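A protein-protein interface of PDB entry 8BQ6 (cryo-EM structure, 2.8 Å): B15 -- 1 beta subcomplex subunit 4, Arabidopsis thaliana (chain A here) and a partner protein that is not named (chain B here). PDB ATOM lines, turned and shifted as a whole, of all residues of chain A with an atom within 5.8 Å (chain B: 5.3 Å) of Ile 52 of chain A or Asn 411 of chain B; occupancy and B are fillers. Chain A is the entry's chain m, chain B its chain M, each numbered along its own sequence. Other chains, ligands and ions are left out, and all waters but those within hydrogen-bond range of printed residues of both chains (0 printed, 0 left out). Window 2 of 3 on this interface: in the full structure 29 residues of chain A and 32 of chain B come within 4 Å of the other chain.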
ATOM      1  N   ILE A  47     -16.794  -4.471 -15.302  1.00  0.00           N
ATOM      2  CA  ILE A  47     -17.145  -4.659 -13.896  1.00  0.00           C
ATOM      3  C   ILE A  47     -17.060  -3.338 -13.140  1.00  0.00           C
ATOM      4  O   ILE A  47     -17.939  -3.011 -12.333  1.00  0.00           O
ATOM      5  CB  ILE A  47     -16.247  -5.740 -13.270  1.00  0.00           C
ATOM      6  CG1 ILE A  47     -16.775  -7.122 -13.651  1.00  0.00           C
ATOM      7  CG2 ILE A  47     -16.176  -5.577 -11.763  1.00  0.00           C
ATOM      8  CD1 ILE A  47     -15.816  -8.234 -13.369  1.00  0.00           C
ATOM      9  N   VAL A  48     -16.013  -2.553 -13.394  1.00  0.00           N
ATOM     10  CA  VAL A  48     -15.886  -1.255 -12.738  1.00  0.00           C
ATOM     11  C   VAL A  48     -16.985  -0.307 -13.198  1.00  0.00           C
ATOM     12  O   VAL A  48     -17.521   0.474 -12.403  1.00  0.00           O
ATOM     13  CB  VAL A  48     -14.484  -0.667 -12.980  1.00  0.00           C
ATOM     14  CG1 VAL A  48     -14.319   0.619 -12.215  1.00  0.00           C
ATOM     15  CG2 VAL A  48     -13.430  -1.652 -12.531  1.00  0.00           C
ATOM     16  N   TYR A  49     -17.331  -0.361 -14.487  1.00  0.00           N
ATOM     17  CA  TYR A  49     -18.402   0.515 -15.025  1.00  0.00           C
ATOM     18  C   TYR A  49     -19.720   0.214 -14.314  1.00  0.00           C
ATOM     19  O   TYR A  49     -20.387   1.168 -13.893  1.00  0.00           O
ATOM     20  CB  TYR A  49     -18.572   0.347 -16.536  1.00  0.00           C
ATOM     21  CG  TYR A  49     -19.621   1.251 -17.131  1.00  0.00           C
ATOM     22  CD1 TYR A  49     -19.332   2.569 -17.440  1.00  0.00           C
ATOM     23  CD2 TYR A  49     -20.910   0.800 -17.362  1.00  0.00           C
ATOM     24  CE1 TYR A  49     -20.291   3.413 -17.976  1.00  0.00           C
ATOM     25  CE2 TYR A  49     -21.883   1.630 -17.890  1.00  0.00           C
ATOM     26  CZ  TYR A  49     -21.572   2.941 -18.199  1.00  0.00           C
ATOM     27  OH  TYR A  49     -22.524   3.763 -18.725  1.00  0.00           O
ATOM     28  N   LYS A  50     -20.073  -1.065 -14.184  1.00  0.00           N
ATOM     29  CA  LYS A  50     -21.350  -1.426 -13.583  1.00  0.00           C
ATOM     30  C   LYS A  50     -21.345  -1.152 -12.087  1.00  0.00           C
ATOM     31  O   LYS A  50     -22.382  -0.808 -11.508  1.00  0.00           O
ATOM     32  CB  LYS A  50     -21.662  -2.892 -13.872  1.00  0.00           C
ATOM     33  CG  LYS A  50     -21.704  -3.208 -15.357  1.00  0.00           C
ATOM     34  CD  LYS A  50     -23.063  -3.726 -15.772  1.00  0.00           C
ATOM     35  CE  LYS A  50     -23.166  -3.847 -17.281  1.00  0.00           C
ATOM     36  NZ  LYS A  50     -24.024  -2.777 -17.863  1.00  0.00           N
ATOM     37  N   GLY A  51     -20.185  -1.294 -11.447  1.00  0.00           N
ATOM     38  CA  GLY A  51     -20.084  -0.944 -10.041  1.00  0.00           C
ATOM     39  C   GLY A  51     -20.318   0.533  -9.796  1.00  0.00           C
ATOM     40  O   GLY A  51     -20.942   0.921  -8.805  1.00  0.00           O
ATOM     41  N   ILE A  52     -19.813   1.382 -10.692  1.00  0.00           N
ATOM     42  CA  ILE A  52     -20.006   2.820 -10.529  1.00  0.00           C
ATOM     43  C   ILE A  52     -21.460   3.198 -10.783  1.00  0.00           C
ATOM     44  O   ILE A  52     -22.045   3.999 -10.043  1.00  0.00           O
ATOM     45  CB  ILE A  52     -19.042   3.600 -11.440  1.00  0.00           C
ATOM     46  CG1 ILE A  52     -17.605   3.437 -10.949  1.00  0.00           C
ATOM     47  CG2 ILE A  52     -19.412   5.069 -11.471  1.00  0.00           C
ATOM     48  CD1 ILE A  52     -16.572   4.025 -11.877  1.00  0.00           C
ATOM     49  N   VAL A  53     -22.042   2.633 -11.842  1.00  0.00           N
ATOM     50  CA  VAL A  53     -23.487   2.869 -12.135  1.00  0.00           C
ATOM     51  C   VAL A  53     -24.317   2.377 -10.943  1.00  0.00           C
ATOM     52  O   VAL A  53     -25.198   3.121 -10.511  1.00  0.00           O
ATOM     53  CB  VAL A  53     -23.899   2.175 -13.446  1.00  0.00           C
ATOM     54  CG1 VAL A  53     -25.398   1.958 -13.562  1.00  0.00           C
ATOM     55  CG2 VAL A  53     -23.383   2.924 -14.662  1.00  0.00           C
ATOM     56  N   LYS A  54     -24.045   1.168 -10.439  1.00  0.00           N
ATOM     57  CA  LYS A  54     -24.825   0.623  -9.333  1.00  0.00           C
ATOM     58  C   LYS A  54     -24.715   1.515  -8.103  1.00  0.00           C
ATOM     59  O   LYS A  54     -25.694   1.702  -7.370  1.00  0.00           O
ATOM     60  CB  LYS A  54     -24.365  -0.801  -9.023  1.00  0.00           C
ATOM     61  CG  LYS A  54     -24.777  -1.344  -7.663  1.00  0.00           C
ATOM     62  CD  LYS A  54     -25.063  -2.837  -7.751  1.00  0.00           C
ATOM     63  CE  LYS A  54     -25.720  -3.366  -6.488  1.00  0.00           C
ATOM     64  NZ  LYS A  54     -24.729  -3.569  -5.396  1.00  0.00           N
ATOM     65  N   ASP A  55     -23.533   2.091  -7.874  1.00  0.00           N
ATOM     66  CA  ASP A  55     -23.348   3.020  -6.766  1.00  0.00           C
ATOM     67  C   ASP A  55     -24.262   4.229  -6.905  1.00  0.00           C
ATOM     68  O   ASP A  55     -24.865   4.685  -5.927  1.00  0.00           O
ATOM     69  CB  ASP A  55     -21.889   3.466  -6.699  1.00  0.00           C
ATOM     70  CG  ASP A  55     -21.450   3.796  -5.295  1.00  0.00           C
ATOM     71  OD1 ASP A  55     -21.424   4.994  -4.943  1.00  0.00           O
ATOM     72  OD2 ASP A  55     -21.119   2.856  -4.547  1.00  0.00           O
ATOM     73  N   PHE A  56     -24.335   4.782  -8.114  1.00  0.00           N
ATOM     74  CA  PHE A  56     -25.265   5.913  -8.348  1.00  0.00           C
ATOM     75  C   PHE A  56     -26.692   5.426  -8.093  1.00  0.00           C
ATOM     76  O   PHE A  56     -27.367   6.046  -7.288  1.00  0.00           O
ATOM     77  CB  PHE A  56     -25.128   6.446  -9.776  1.00  0.00           C
ATOM     78  CG  PHE A  56     -23.951   7.356 -10.014  1.00  0.00           C
ATOM     79  CD1 PHE A  56     -23.761   8.488  -9.239  1.00  0.00           C
ATOM     80  CD2 PHE A  56     -23.044   7.091 -11.027  1.00  0.00           C
ATOM     81  CE1 PHE A  56     -22.680   9.325  -9.464  1.00  0.00           C
ATOM     82  CE2 PHE A  56     -21.967   7.932 -11.252  1.00  0.00           C
ATOM     83  CZ  PHE A  56     -21.786   9.046 -10.470  1.00  0.00           C
ATOM     84  N   HIS A  57     -27.102   4.325  -8.721  1.00  0.00           N
ATOM     85  CA  HIS A  57     -28.493   3.809  -8.611  1.00  0.00           C
ATOM     86  C   HIS A  57     -28.896   3.554  -7.154  1.00  0.00           C
ATOM     87  O   HIS A  57     -30.028   3.893  -6.819  1.00  0.00           O
ATOM     88  CB  HIS A  57     -28.644   2.561  -9.486  1.00  0.00           C
ATOM     89  CG  HIS A  57     -28.718   2.862 -10.944  1.00  0.00           C
ATOM     90  ND1 HIS A  57     -28.854   1.870 -11.891  1.00  0.00           N
ATOM     91  CD2 HIS A  57     -28.685   4.030 -11.619  1.00  0.00           C
ATOM     92  CE1 HIS A  57     -28.906   2.414 -13.089  1.00  0.00           C
ATOM     93  NE2 HIS A  57     -28.798   3.736 -12.949  1.00  0.00           N
ATOM     94  N   GLN A  59     -27.842   5.084  -4.602  1.00  0.00           N
ATOM     95  CA  GLN A  59     -28.124   6.406  -4.056  1.00  0.00           C
ATOM     96  C   GLN A  59     -29.508   6.886  -4.477  1.00  0.00           C
ATOM     97  O   GLN A  59     -30.217   7.517  -3.685  1.00  0.00           O
ATOM     98  CB  GLN A  59     -27.062   7.410  -4.506  1.00  0.00           C
ATOM     99  CG  GLN A  59     -25.663   7.187  -3.958  1.00  0.00           C
ATOM    100  CD  GLN A  59     -24.618   7.952  -4.753  1.00  0.00           C
ATOM    101  OE1 GLN A  59     -24.953   8.756  -5.622  1.00  0.00           O
ATOM    102  NE2 GLN A  59     -23.347   7.701  -4.464  1.00  0.00           N
ATOM    103  N   PRO B 281     -20.366   8.135 -15.333  1.00  0.00           N
ATOM    104  CA  PRO B 281     -19.840   6.797 -15.042  1.00  0.00           C
ATOM    105  C   PRO B 281     -18.788   6.390 -16.087  1.00  0.00           C
ATOM    106  O   PRO B 281     -17.869   5.702 -15.722  1.00  0.00           O
ATOM    107  CB  PRO B 281     -21.030   5.845 -15.132  1.00  0.00           C
ATOM    108  CG  PRO B 281     -22.190   6.715 -14.785  1.00  0.00           C
ATOM    109  CD  PRO B 281     -21.847   8.026 -15.453  1.00  0.00           C
ATOM    110  N   TYR B 284     -15.589   8.204 -15.194  1.00  0.00           N
ATOM    111  CA  TYR B 284     -15.089   7.651 -13.941  1.00  0.00           C
ATOM    112  C   TYR B 284     -14.387   6.319 -14.172  1.00  0.00           C
ATOM    113  O   TYR B 284     -13.330   6.051 -13.590  1.00  0.00           O
ATOM    114  CB  TYR B 284     -16.239   7.491 -12.946  1.00  0.00           C
ATOM    115  CG  TYR B 284     -16.588   8.755 -12.199  1.00  0.00           C
ATOM    116  CD1 TYR B 284     -15.744   9.852 -12.229  1.00  0.00           C
ATOM    117  CD2 TYR B 284     -17.749   8.841 -11.444  1.00  0.00           C
ATOM    118  CE1 TYR B 284     -16.049  11.002 -11.543  1.00  0.00           C
ATOM    119  CE2 TYR B 284     -18.061   9.989 -10.751  1.00  0.00           C
ATOM    120  CZ  TYR B 284     -17.207  11.066 -10.806  1.00  0.00           C
ATOM    121  OH  TYR B 284     -17.507  12.215 -10.119  1.00  0.00           O
ATOM    122  N   THR B 285     -14.958   5.472 -15.030  1.00  0.00           N
ATOM    123  CA  THR B 285     -14.363   4.169 -15.301  1.00  0.00           C
ATOM    124  C   THR B 285     -13.027   4.303 -16.024  1.00  0.00           C
ATOM    125  O   THR B 285     -12.041   3.660 -15.649  1.00  0.00           O
ATOM    126  CB  THR B 285     -15.327   3.313 -16.120  1.00  0.00           C
ATOM    127  OG1 THR B 285     -16.597   3.268 -15.462  1.00  0.00           O
ATOM    128  CG2 THR B 285     -14.786   1.905 -16.276  1.00  0.00           C
ATOM    129  N   ALA B 407     -14.869  13.803  -5.266  1.00  0.00           N
ATOM    130  CA  ALA B 407     -15.303  12.518  -5.801  1.00  0.00           C
ATOM    131  C   ALA B 407     -16.082  11.725  -4.762  1.00  0.00           C
ATOM    132  O   ALA B 407     -17.050  11.034  -5.097  1.00  0.00           O
ATOM    133  CB  ALA B 407     -14.098  11.719  -6.293  1.00  0.00           C
ATOM    134  N   PHE B 408     -15.673  11.815  -3.497  1.00  0.00           N
ATOM    135  CA  PHE B 408     -16.348  11.075  -2.438  1.00  0.00           C
ATOM    136  C   PHE B 408     -17.783  11.547  -2.256  1.00  0.00           C
ATOM    137  O   PHE B 408     -18.674  10.748  -1.946  1.00  0.00           O
ATOM    138  CB  PHE B 408     -15.571  11.218  -1.133  1.00  0.00           C
ATOM    139  CG  PHE B 408     -15.875  10.151  -0.138  1.00  0.00           C
ATOM    140  CD1 PHE B 408     -15.122   8.995  -0.098  1.00  0.00           C
ATOM    141  CD2 PHE B 408     -16.921  10.297   0.753  1.00  0.00           C
ATOM    142  CE1 PHE B 408     -15.402   8.007   0.818  1.00  0.00           C
ATOM    143  CE2 PHE B 408     -17.204   9.312   1.670  1.00  0.00           C
ATOM    144  CZ  PHE B 408     -16.444   8.167   1.702  1.00  0.00           C
ATOM    145  N   GLN B 409     -18.027  12.845  -2.434  1.00  0.00           N
ATOM    146  CA  GLN B 409     -19.376  13.375  -2.294  1.00  0.00           C
ATOM    147  C   GLN B 409     -20.289  12.979  -3.444  1.00  0.00           C
ATOM    148  O   GLN B 409     -21.502  13.189  -3.351  1.00  0.00           O
ATOM    149  CB  GLN B 409     -19.336  14.893  -2.194  1.00  0.00           C
ATOM    150  CG  GLN B 409     -18.537  15.416  -1.040  1.00  0.00           C
ATOM    151  CD  GLN B 409     -18.649  16.912  -0.934  1.00  0.00           C
ATOM    152  OE1 GLN B 409     -19.466  17.533  -1.607  1.00  0.00           O
ATOM    153  NE2 GLN B 409     -17.811  17.502  -0.109  1.00  0.00           N
ATOM    154  N   ARG B 410     -19.744  12.440  -4.532  1.00  0.00           N
ATOM    155  CA  ARG B 410     -20.565  11.969  -5.640  1.00  0.00           C
ATOM    156  C   ARG B 410     -20.635  10.452  -5.706  1.00  0.00           C
ATOM    157  O   ARG B 410     -21.728   9.881  -5.722  1.00  0.00           O
ATOM    158  CB  ARG B 410     -20.035  12.519  -6.968  1.00  0.00           C
ATOM    159  CG  ARG B 410     -19.924  14.017  -6.980  1.00  0.00           C
ATOM    160  CD  ARG B 410     -21.221  14.707  -7.400  1.00  0.00           C
ATOM    161  NE  ARG B 410     -21.445  14.721  -8.842  1.00  0.00           N
ATOM    162  CZ  ARG B 410     -21.934  13.716  -9.556  1.00  0.00           C
ATOM    163  NH1 ARG B 410     -22.345  12.594  -8.990  1.00  0.00           N
ATOM    164  NH2 ARG B 410     -22.014  13.841 -10.878  1.00  0.00           N
ATOM    165  N   ASN B 411     -19.486   9.788  -5.746  1.00  0.00           N
ATOM    166  CA  ASN B 411     -19.451   8.335  -5.832  1.00  0.00           C
ATOM    167  C   ASN B 411     -18.304   7.847  -4.962  1.00  0.00           C
ATOM    168  O   ASN B 411     -17.145   8.181  -5.219  1.00  0.00           O
ATOM    169  CB  ASN B 411     -19.281   7.879  -7.274  1.00  0.00           C
ATOM    170  CG  ASN B 411     -19.905   6.535  -7.526  1.00  0.00           C
ATOM    171  OD1 ASN B 411     -19.314   5.499  -7.231  1.00  0.00           O
ATOM    172  ND2 ASN B 411     -21.116   6.540  -8.061  1.00  0.00           N
ATOM    173  N   SER B 412     -18.624   7.056  -3.939  1.00  0.00           N
ATOM    174  CA  SER B 412     -17.589   6.643  -3.001  1.00  0.00           C
ATOM    175  C   SER B 412     -16.691   5.569  -3.601  1.00  0.00           C
ATOM    176  O   SER B 412     -15.561   5.371  -3.142  1.00  0.00           O
ATOM    177  CB  SER B 412     -18.225   6.157  -1.701  1.00  0.00           C
ATOM    178  OG  SER B 412     -18.452   4.763  -1.740  1.00  0.00           O
ATOM    179  N   LEU B 413     -17.173   4.862  -4.624  1.00  0.00           N
ATOM    180  CA  LEU B 413     -16.358   3.824  -5.245  1.00  0.00           C
ATOM    181  C   LEU B 413     -15.232   4.418  -6.085  1.00  0.00           C
ATOM    182  O   LEU B 413     -14.085   3.965  -6.009  1.00  0.00           O
ATOM    183  CB  LEU B 413     -17.228   2.907  -6.098  1.00  0.00           C
ATOM    184  CG  LEU B 413     -16.449   1.787  -6.788  1.00  0.00           C
ATOM    185  CD1 LEU B 413     -15.782   0.865  -5.778  1.00  0.00           C
ATOM    186  CD2 LEU B 413     -17.366   1.019  -7.702  1.00  0.00           C
ATOM    187  N   VAL B 414     -15.541   5.425  -6.906  1.00  0.00           N
ATOM    188  CA  VAL B 414     -14.505   6.017  -7.752  1.00  0.00           C
ATOM    189  C   VAL B 414     -13.479   6.756  -6.901  1.00  0.00           C
ATOM    190  O   VAL B 414     -12.279   6.740  -7.198  1.00  0.00           O
ATOM    191  CB  VAL B 414     -15.126   6.925  -8.832  1.00  0.00           C
ATOM    192  CG1 VAL B 414     -15.898   8.067  -8.216  1.00  0.00           C
ATOM    193  CG2 VAL B 414     -14.045   7.461  -9.758  1.00  0.00           C
ATOM    194  N   ALA B 415     -13.926   7.404  -5.822  1.00  0.00           N
ATOM    195  CA  ALA B 415     -12.985   8.041  -4.907  1.00  0.00           C
ATOM    196  C   ALA B 415     -12.088   7.010  -4.232  1.00  0.00           C
ATOM    197  O   ALA B 415     -10.948   7.313  -3.862  1.00  0.00           O
ATOM    198  CB  ALA B 415     -13.737   8.858  -3.859  1.00  0.00           C
ATOM    199  N   THR B 416     -12.594   5.788  -4.041  1.00  0.00           N
ATOM    200  CA  THR B 416     -11.788   4.741  -3.422  1.00  0.00           C
ATOM    201  C   THR B 416     -10.736   4.209  -4.383  1.00  0.00           C
ATOM    202  O   THR B 416      -9.578   4.003  -3.999  1.00  0.00           O
ATOM    203  CB  THR B 416     -12.683   3.598  -2.946  1.00  0.00           C
ATOM    204  OG1 THR B 416     -13.477   4.038  -1.840  1.00  0.00           O
ATOM    205  CG2 THR B 416     -11.843   2.409  -2.519  1.00  0.00           C
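CA of Tyr 49 of chain A touches OG1 of Thr 285 of chain B, 3.3 Å away. Leu 413 of chain B touches Gly 51 of chain A (CD2 to C, 3.7 Å). Pro 281 of chain B touches Ile 52 of chain A. Ile 52 of chain A touches Tyr 284 of chain B (CD1 to CB, 3.6 Å). CD1 of Ile 52 of chain A touches OG1 of Thr 285 of chain B (3.7 Å). Ile 52 of chain A touches Leu 413 of chain B. Asp 55 of chain A touches Ser 412 of chain B. CG of Pro 281 of chain B touches CE2 of Phe 56 of chain A, 3.7 Å away. Phe 56 of chain A touches Arg 410 of chain B (CE1 to NH1, 3.3 Å). Phe 56 of chain A touches Asn 411 of chain B (CE1 to ND2, 3.5 Å).
Hydrophobic or aromatic side chains of chain B that line the printed part of chain A: Pro 281, Tyr 284 and Leu 413. Of the 12 printed residues of chain A, 7 touch a printed residue of chain B. Along chain A the printed residues that touch a printed residue of chain B span positions 49 to 59. Among the printed residues, no Asp or Glu carboxylate lies within 4 Å of a Lys or Arg side-chain nitrogen of the other chain.
Asn 411 of chain B touches just these residues of chain A: Ile 52, Asp 55 and Phe 56. Of the printed residues of chain B, Val 53 of chain A touches Pro 281 (3.8 Å). Of the printed residues of chain A, Thr 285 of chain B touches Tyr 49 (3.3 Å) and Ile 52 (3.7 Å). Printed residues of chain B within 4 Å of Asp 55 of chain A: Asn 411 (3.2 Å) and Ser 412 (3.6 Å). Of the printed residues of chain A, Ser 412 of chain B touches Asp 55 (3.6 Å). The nearest residue of chain A that does not touch Asn 411 of chain B is Gln 59 of chain A (4.2 Å).
OG1 of Thr 416 of chain B sits at hydrogen-bond distance from O of Ser 412 of chain B, 2.8 Å away. The backbone carbonyl oxygen (O) of Pro 281 of chain B is in hydrogen-bond range of the side-chain hydroxyl (OG1) of Thr 285 of chain B (2.8 Å). OD1 of Asp 55 of chain A is in hydrogen-bond range of NE2 of Gln 59 of chain A, at 3.4 Å. The side-chain amide oxygen (OD1) of Asn 411 of chain B lies close to the backbone NH (N) of Leu 413 of chain B, 3.4 Å away.
The side-chain amide nitrogen (ND2) of Asn 411 of chain B sits at hydrogen-bond distance from the backbone carbonyl oxygen (O) of Ile 52 of chain A. The side-chain amide oxygen (OD1) of Asn 411 of chain B sits close to the side-chain carboxylate (OD1) of Asp 55 of chain A. The side-chain amide nitrogen (NE2) of Gln 59 of chain A lies within hydrogen-bond range of the backbone carbonyl oxygen (O) of Arg 410 of chain B.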
